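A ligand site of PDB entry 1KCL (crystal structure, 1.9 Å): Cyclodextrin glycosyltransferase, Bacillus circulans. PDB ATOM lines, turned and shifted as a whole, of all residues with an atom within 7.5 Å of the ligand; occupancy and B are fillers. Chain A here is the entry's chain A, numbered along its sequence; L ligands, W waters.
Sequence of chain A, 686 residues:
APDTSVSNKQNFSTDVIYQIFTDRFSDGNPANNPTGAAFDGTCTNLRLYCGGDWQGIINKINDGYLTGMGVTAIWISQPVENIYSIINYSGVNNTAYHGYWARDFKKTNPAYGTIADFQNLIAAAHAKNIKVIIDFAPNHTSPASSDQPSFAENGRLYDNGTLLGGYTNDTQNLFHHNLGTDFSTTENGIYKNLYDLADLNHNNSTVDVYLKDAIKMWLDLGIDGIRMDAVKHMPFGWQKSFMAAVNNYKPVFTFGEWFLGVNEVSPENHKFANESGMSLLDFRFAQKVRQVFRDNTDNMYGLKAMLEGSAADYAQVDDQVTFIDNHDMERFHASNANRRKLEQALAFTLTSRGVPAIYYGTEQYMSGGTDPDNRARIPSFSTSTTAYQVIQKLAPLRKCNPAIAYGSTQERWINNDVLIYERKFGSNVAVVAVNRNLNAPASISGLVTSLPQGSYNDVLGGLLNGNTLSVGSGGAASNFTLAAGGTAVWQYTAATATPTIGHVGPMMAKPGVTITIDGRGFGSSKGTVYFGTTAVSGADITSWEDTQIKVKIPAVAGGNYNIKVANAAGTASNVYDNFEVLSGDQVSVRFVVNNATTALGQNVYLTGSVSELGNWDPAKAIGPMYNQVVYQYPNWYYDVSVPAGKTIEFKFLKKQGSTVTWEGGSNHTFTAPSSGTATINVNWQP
OD2 of Asp 295 lies within hydrogen-bond range of O2 of the ligand, at 2.6 Å.
OE1 of Glu 330 sits at hydrogen-bond distance from O1 of the ligand, at 2.7 Å.
NE of Arg 290 lies within hydrogen-bond range of O2 of the ligand (2.8 Å).
The side-chain amide oxygen (OE1) of Gln 287 lies within hydrogen-bond range of an oxygen (O3) of the ligand (2.9 Å).
O2 of the ligand lies within hydrogen-bond range of NH1 of Arg 294 (3.3 Å).
The backbone NH (N) of Asp 295 sits at hydrogen-bond distance from the backbone carbonyl oxygen (O) of Arg 290 (2.7 Å).
OD1 of Asp 295 is in salt-bridge range of NH1 of Arg 294, 2.7 Å away.
NH2 of Arg 290 is in hydrogen-bond range of O of Glu 330 (3.1 Å).
The guanidinium group (NH1) of Arg 290 sits at hydrogen-bond distance from the backbone carbonyl oxygen (O) of Ile 324 (2.8 Å).
O of Leu 260 lies within hydrogen-bond range of NE2 of Gln 287 (2.8 Å).
The backbone carbonyl oxygen (O) of Arg 331 is in hydrogen-bond range of the guanidinium group (NH2) of Arg 294 (3.1 Å).
The guanidinium group (NE) of Arg 294 sits at hydrogen-bond distance from the backbone carbonyl oxygen (O) of Phe 332.
CG2 of Val 262 touches O3 of the ligand, 3.4 Å away.
Of the 20 residues printed, 6 come within 4 Å of the ligand.
Water W3 lies within hydrogen-bond range of an oxygen (O1) of the ligand and the backbone NH (N) of Glu 330.
Water W2 bridges N of Val 262 and O4 of the ligand.
Water W4 bridges OD2 of Asp 295 (2.6 Å) and O3 of the ligand (2.9 Å).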
ATOM      1  N   PHE A 259      -3.200   0.399  29.358  1.00  0.00           N
ATOM      2  CA  PHE A 259      -3.175   1.004  28.044  1.00  0.00           C
ATOM      3  C   PHE A 259      -2.304   0.266  27.033  1.00  0.00           C
ATOM      4  O   PHE A 259      -1.175  -0.137  27.322  1.00  0.00           O
ATOM      5  CB  PHE A 259      -2.721   2.468  28.146  1.00  0.00           C
ATOM      6  CG  PHE A 259      -2.988   3.285  26.906  1.00  0.00           C
ATOM      7  CD1 PHE A 259      -2.249   3.082  25.748  1.00  0.00           C
ATOM      8  CD2 PHE A 259      -4.002   4.237  26.902  1.00  0.00           C
ATOM      9  CE1 PHE A 259      -2.514   3.811  24.591  1.00  0.00           C
ATOM     10  CE2 PHE A 259      -4.281   4.970  25.743  1.00  0.00           C
ATOM     11  CZ  PHE A 259      -3.533   4.747  24.590  1.00  0.00           C
ATOM     12  N   LEU A 260      -2.855   0.075  25.829  1.00  0.00           N
ATOM     13  CA  LEU A 260      -2.150  -0.560  24.721  1.00  0.00           C
ATOM     14  C   LEU A 260      -2.300   0.354  23.516  1.00  0.00           C
ATOM     15  O   LEU A 260      -3.382   0.861  23.246  1.00  0.00           O
ATOM     16  CB  LEU A 260      -2.748  -1.930  24.396  1.00  0.00           C
ATOM     17  CG  LEU A 260      -2.615  -3.045  25.438  1.00  0.00           C
ATOM     18  CD1 LEU A 260      -3.357  -4.274  24.938  1.00  0.00           C
ATOM     19  CD2 LEU A 260      -1.147  -3.362  25.690  1.00  0.00           C
ATOM     20  N   GLY A 261      -1.207   0.558  22.787  1.00  0.00           N
ATOM     21  CA  GLY A 261      -1.261   1.406  21.609  1.00  0.00           C
ATOM     22  C   GLY A 261      -1.614   0.610  20.362  1.00  0.00           C
ATOM     23  O   GLY A 261      -1.818  -0.605  20.431  1.00  0.00           O
ATOM     24  N   VAL A 262      -1.701   1.304  19.235  1.00  0.00           N
ATOM     25  CA  VAL A 262      -2.030   0.644  17.971  1.00  0.00           C
ATOM     26  C   VAL A 262      -1.008  -0.453  17.685  1.00  0.00           C
ATOM     27  O   VAL A 262       0.194  -0.263  17.855  1.00  0.00           O
ATOM     28  CB  VAL A 262      -2.023   1.661  16.791  1.00  0.00           C
ATOM     29  CG1 VAL A 262      -2.295   0.943  15.478  1.00  0.00           C
ATOM     30  CG2 VAL A 262      -3.072   2.741  17.027  1.00  0.00           C
ATOM     31  N   ALA A 286     -10.244  -2.104  21.085  1.00  0.00           N
ATOM     32  CA  ALA A 286     -10.490  -0.696  20.795  1.00  0.00           C
ATOM     33  C   ALA A 286      -9.596  -0.127  19.701  1.00  0.00           C
ATOM     34  O   ALA A 286     -10.087   0.511  18.770  1.00  0.00           O
ATOM     35  CB  ALA A 286     -10.341   0.125  22.069  1.00  0.00           C
ATOM     36  N   GLN A 287      -8.294  -0.365  19.810  1.00  0.00           N
ATOM     37  CA  GLN A 287      -7.336   0.139  18.826  1.00  0.00           C
ATOM     38  C   GLN A 287      -7.566  -0.437  17.435  1.00  0.00           C
ATOM     39  O   GLN A 287      -7.481   0.276  16.435  1.00  0.00           O
ATOM     40  CB  GLN A 287      -5.900  -0.164  19.285  1.00  0.00           C
ATOM     41  CG  GLN A 287      -5.509   0.509  20.608  1.00  0.00           C
ATOM     42  CD  GLN A 287      -5.357   2.021  20.479  1.00  0.00           C
ATOM     43  OE1 GLN A 287      -5.980   2.645  19.620  1.00  0.00           O
ATOM     44  NE2 GLN A 287      -4.559   2.613  21.364  1.00  0.00           N
ATOM     45  N   LYS A 288      -7.876  -1.734  17.364  1.00  0.00           N
ATOM     46  CA  LYS A 288      -8.126  -2.382  16.081  1.00  0.00           C
ATOM     47  C   LYS A 288      -9.408  -1.841  15.451  1.00  0.00           C
ATOM     48  O   LYS A 288      -9.469  -1.618  14.232  1.00  0.00           O
ATOM     49  CB  LYS A 288      -8.226  -3.898  16.257  1.00  0.00           C
ATOM     50  CG  LYS A 288      -8.394  -4.669  14.946  1.00  0.00           C
ATOM     51  CD  LYS A 288      -7.249  -4.393  13.980  1.00  0.00           C
ATOM     52  CE  LYS A 288      -5.897  -4.815  14.551  1.00  0.00           C
ATOM     53  NZ  LYS A 288      -4.769  -4.492  13.639  1.00  0.00           N
ATOM     54  N   VAL A 289     -10.439  -1.636  16.264  1.00  0.00           N
ATOM     55  CA  VAL A 289     -11.703  -1.090  15.780  1.00  0.00           C
ATOM     56  C   VAL A 289     -11.483   0.301  15.182  1.00  0.00           C
ATOM     57  O   VAL A 289     -12.069   0.648  14.159  1.00  0.00           O
ATOM     58  CB  VAL A 289     -12.762  -1.016  16.911  1.00  0.00           C
ATOM     59  CG1 VAL A 289     -13.969  -0.186  16.459  1.00  0.00           C
ATOM     60  CG2 VAL A 289     -13.221  -2.418  17.289  1.00  0.00           C
ATOM     61  N   ARG A 290     -10.645   1.092  15.844  1.00  0.00           N
ATOM     62  CA  ARG A 290     -10.327   2.439  15.366  1.00  0.00           C
ATOM     63  C   ARG A 290      -9.555   2.359  14.049  1.00  0.00           C
ATOM     64  O   ARG A 290      -9.792   3.149  13.126  1.00  0.00           O
ATOM     65  CB  ARG A 290      -9.519   3.203  16.410  1.00  0.00           C
ATOM     66  CG  ARG A 290     -10.291   3.492  17.706  1.00  0.00           C
ATOM     67  CD  ARG A 290      -9.401   4.148  18.753  1.00  0.00           C
ATOM     68  NE  ARG A 290      -9.042   5.522  18.403  1.00  0.00           N
ATOM     69  CZ  ARG A 290      -9.720   6.604  18.787  1.00  0.00           C
ATOM     70  NH1 ARG A 290     -10.806   6.469  19.552  1.00  0.00           N
ATOM     71  NH2 ARG A 290      -9.323   7.808  18.420  1.00  0.00           N
ATOM     72  N   GLN A 291      -8.631   1.402  13.945  1.00  0.00           N
ATOM     73  CA  GLN A 291      -7.845   1.210  12.736  1.00  0.00           C
ATOM     74  C   GLN A 291      -8.722   0.859  11.548  1.00  0.00           C
ATOM     75  O   GLN A 291      -8.534   1.375  10.441  1.00  0.00           O
ATOM     76  CB  GLN A 291      -6.838   0.073  12.910  1.00  0.00           C
ATOM     77  CG  GLN A 291      -5.560   0.437  13.627  1.00  0.00           C
ATOM     78  CD  GLN A 291      -4.547  -0.686  13.568  1.00  0.00           C
ATOM     79  OE1 GLN A 291      -4.736  -1.741  14.171  1.00  0.00           O
ATOM     80  NE2 GLN A 291      -3.476  -0.474  12.803  1.00  0.00           N
ATOM     81  N   ARG A 294     -12.249   3.786  11.831  1.00  0.00           N
ATOM     82  CA  ARG A 294     -11.970   5.212  11.947  1.00  0.00           C
ATOM     83  C   ARG A 294     -10.805   5.747  11.129  1.00  0.00           C
ATOM     84  O   ARG A 294     -10.968   6.696  10.352  1.00  0.00           O
ATOM     85  CB  ARG A 294     -11.731   5.565  13.424  1.00  0.00           C
ATOM     86  CG  ARG A 294     -11.459   7.047  13.705  1.00  0.00           C
ATOM     87  CD  ARG A 294     -11.197   7.238  15.187  1.00  0.00           C
ATOM     88  NE  ARG A 294     -11.187   8.642  15.610  1.00  0.00           N
ATOM     89  CZ  ARG A 294     -10.192   9.496  15.414  1.00  0.00           C
ATOM     90  NH1 ARG A 294      -9.087   9.109  14.783  1.00  0.00           N
ATOM     91  NH2 ARG A 294     -10.283  10.732  15.863  1.00  0.00           N
ATOM     92  N   ASP A 295      -9.638   5.136  11.277  1.00  0.00           N
ATOM     93  CA  ASP A 295      -8.423   5.616  10.629  1.00  0.00           C
ATOM     94  C   ASP A 295      -7.992   4.918   9.345  1.00  0.00           C
ATOM     95  O   ASP A 295      -7.000   5.320   8.724  1.00  0.00           O
ATOM     96  CB  ASP A 295      -7.290   5.595  11.643  1.00  0.00           C
ATOM     97  CG  ASP A 295      -7.681   6.236  12.955  1.00  0.00           C
ATOM     98  OD1 ASP A 295      -8.167   7.388  12.943  1.00  0.00           O
ATOM     99  OD2 ASP A 295      -7.506   5.588  14.013  1.00  0.00           O
ATOM    100  N   THR A 297      -6.430   2.121   8.683  1.00  0.00           N
ATOM    101  CA  THR A 297      -5.059   1.640   8.676  1.00  0.00           C
ATOM    102  C   THR A 297      -4.992   0.112   8.741  1.00  0.00           C
ATOM    103  O   THR A 297      -3.920  -0.466   8.892  1.00  0.00           O
ATOM    104  CB  THR A 297      -4.216   2.231   9.827  1.00  0.00           C
ATOM    105  OG1 THR A 297      -4.862   1.977  11.079  1.00  0.00           O
ATOM    106  CG2 THR A 297      -4.057   3.741   9.641  1.00  0.00           C
ATOM    107  N   ILE A 324     -14.675   2.031  21.974  1.00  0.00           N
ATOM    108  CA  ILE A 324     -14.104   2.600  20.757  1.00  0.00           C
ATOM    109  C   ILE A 324     -13.318   3.867  21.069  1.00  0.00           C
ATOM    110  O   ILE A 324     -12.595   4.391  20.217  1.00  0.00           O
ATOM    111  CB  ILE A 324     -15.194   2.892  19.696  1.00  0.00           C
ATOM    112  CG1 ILE A 324     -16.111   4.025  20.145  1.00  0.00           C
ATOM    113  CG2 ILE A 324     -16.017   1.631  19.445  1.00  0.00           C
ATOM    114  CD1 ILE A 324     -17.176   4.383  19.135  1.00  0.00           C
ATOM    115  N   ASP A 328      -8.844   8.914  27.595  1.00  0.00           N
ATOM    116  CA  ASP A 328      -7.423   8.973  27.263  1.00  0.00           C
ATOM    117  C   ASP A 328      -7.161   8.801  25.772  1.00  0.00           C
ATOM    118  O   ASP A 328      -6.045   8.508  25.353  1.00  0.00           O
ATOM    119  CB  ASP A 328      -6.649   7.903  28.030  1.00  0.00           C
ATOM    120  CG  ASP A 328      -6.675   8.128  29.521  1.00  0.00           C
ATOM    121  OD1 ASP A 328      -6.433   9.275  29.958  1.00  0.00           O
ATOM    122  OD2 ASP A 328      -6.940   7.165  30.265  1.00  0.00           O
ATOM    123  N   MET A 329      -8.203   8.995  24.975  1.00  0.00           N
ATOM    124  CA  MET A 329      -8.101   8.886  23.529  1.00  0.00           C
ATOM    125  C   MET A 329      -8.907  10.001  22.869  1.00  0.00           C
ATOM    126  O   MET A 329      -9.839  10.529  23.481  1.00  0.00           O
ATOM    127  CB  MET A 329      -8.662   7.542  23.043  1.00  0.00           C
ATOM    128  CG  MET A 329      -8.013   6.316  23.662  1.00  0.00           C
ATOM    129  SD  MET A 329      -8.752   4.826  22.997  1.00  0.00           S
ATOM    130  CE  MET A 329      -7.729   4.571  21.556  1.00  0.00           C
ATOM    131  N   GLU A 330      -8.542  10.350  21.646  1.00  0.00           N
ATOM    132  CA  GLU A 330      -9.284  11.366  20.919  1.00  0.00           C
ATOM    133  C   GLU A 330     -10.657  10.767  20.656  1.00  0.00           C
ATOM    134  O   GLU A 330     -10.777   9.559  20.451  1.00  0.00           O
ATOM    135  CB  GLU A 330      -8.617  11.676  19.573  1.00  0.00           C
ATOM    136  CG  GLU A 330      -7.186  12.170  19.695  1.00  0.00           C
ATOM    137  CD  GLU A 330      -6.560  12.429  18.336  1.00  0.00           C
ATOM    138  OE1 GLU A 330      -6.443  11.471  17.539  1.00  0.00           O
ATOM    139  OE2 GLU A 330      -6.195  13.592  18.066  1.00  0.00           O
ATOM    140  N   ARG A 331     -11.693  11.604  20.692  1.00  0.00           N
ATOM    141  CA  ARG A 331     -13.045  11.137  20.421  1.00  0.00           C
ATOM    142  C   ARG A 331     -13.067  10.400  19.086  1.00  0.00           C
ATOM    143  O   ARG A 331     -12.469  10.861  18.110  1.00  0.00           O
ATOM    144  CB  ARG A 331     -14.011  12.325  20.377  1.00  0.00           C
ATOM    145  CG  ARG A 331     -14.266  12.974  21.730  1.00  0.00           C
ATOM    146  CD  ARG A 331     -15.313  12.203  22.519  1.00  0.00           C
ATOM    147  NE  ARG A 331     -15.656  12.859  23.772  1.00  0.00           N
ATOM    148  CZ  ARG A 331     -16.692  12.522  24.529  1.00  0.00           C
ATOM    149  NH1 ARG A 331     -17.492  11.530  24.155  1.00  0.00           N
ATOM    150  NH2 ARG A 331     -16.940  13.168  25.664  1.00  0.00           N
ATOM    151  N   PHE A 332     -13.740   9.253  19.049  1.00  0.00           N
ATOM    152  CA  PHE A 332     -13.804   8.450  17.831  1.00  0.00           C
ATOM    153  C   PHE A 332     -14.327   9.248  16.639  1.00  0.00           C
ATOM    154  O   PHE A 332     -13.784   9.168  15.536  1.00  0.00           O
ATOM    155  CB  PHE A 332     -14.692   7.219  18.063  1.00  0.00           C
ATOM    156  CG  PHE A 332     -14.764   6.289  16.870  1.00  0.00           C
ATOM    157  CD1 PHE A 332     -15.512   6.616  15.747  1.00  0.00           C
ATOM    158  CD2 PHE A 332     -14.054   5.085  16.871  1.00  0.00           C
ATOM    159  CE1 PHE A 332     -15.574   5.766  14.644  1.00  0.00           C
ATOM    160  CE2 PHE A 332     -14.103   4.231  15.769  1.00  0.00           C
ATOM    161  CZ  PHE A 332     -14.865   4.569  14.660  1.00  0.00           C
ATOM    162  N   THR A 370      -7.036  15.006  22.286  1.00  0.00           N
ATOM    163  CA  THR A 370      -6.590  14.424  23.544  1.00  0.00           C
ATOM    164  C   THR A 370      -6.936  15.311  24.739  1.00  0.00           C
ATOM    165  O   THR A 370      -7.302  16.478  24.582  1.00  0.00           O
ATOM    166  CB  THR A 370      -5.072  14.160  23.537  1.00  0.00           C
ATOM    167  OG1 THR A 370      -4.385  15.403  23.337  1.00  0.00           O
ATOM    168  CG2 THR A 370      -4.706  13.199  22.425  1.00  0.00           C
HETATM  169  C1  LIG L   1      -5.759   8.242  16.718  1.00  0.00           C
HETATM  170  C2  LIG L   1      -6.142   6.778  16.532  1.00  0.00           C
HETATM  171  C3  LIG L   1      -5.677   5.937  17.733  1.00  0.00           C
HETATM  172  C4  LIG L   1      -4.188   6.164  17.989  1.00  0.00           C
HETATM  173  C5  LIG L   1      -3.914   7.666  18.130  1.00  0.00           C
HETATM  174  C6  LIG L   1      -2.438   7.980  18.323  1.00  0.00           C
HETATM  175  O1  LIG L   1      -6.420   8.768  17.829  1.00  0.00           O
HETATM  176  O2  LIG L   1      -7.550   6.662  16.388  1.00  0.00           O
HETATM  177  O3  LIG L   1      -5.915   4.569  17.485  1.00  0.00           O
HETATM  178  O4  LIG L   1      -3.788   5.484  19.173  1.00  0.00           O
HETATM  179  O5  LIG L   1      -4.347   8.361  16.945  1.00  0.00           O
HETATM  180  O6  LIG L   1      -1.691   7.642  17.169  1.00  0.00           O
HETATM  181  O   HOH W   1      -4.759   6.149  21.527  1.00  0.00           O
HETATM  182  O   HOH W   2      -1.277   4.119  19.354  1.00  0.00           O
HETATM  183  O   HOH W   3      -6.292   8.306  20.456  1.00  0.00           O
HETATM  184  O   HOH W   4      -5.889   3.668  14.719  1.00  0.00           O
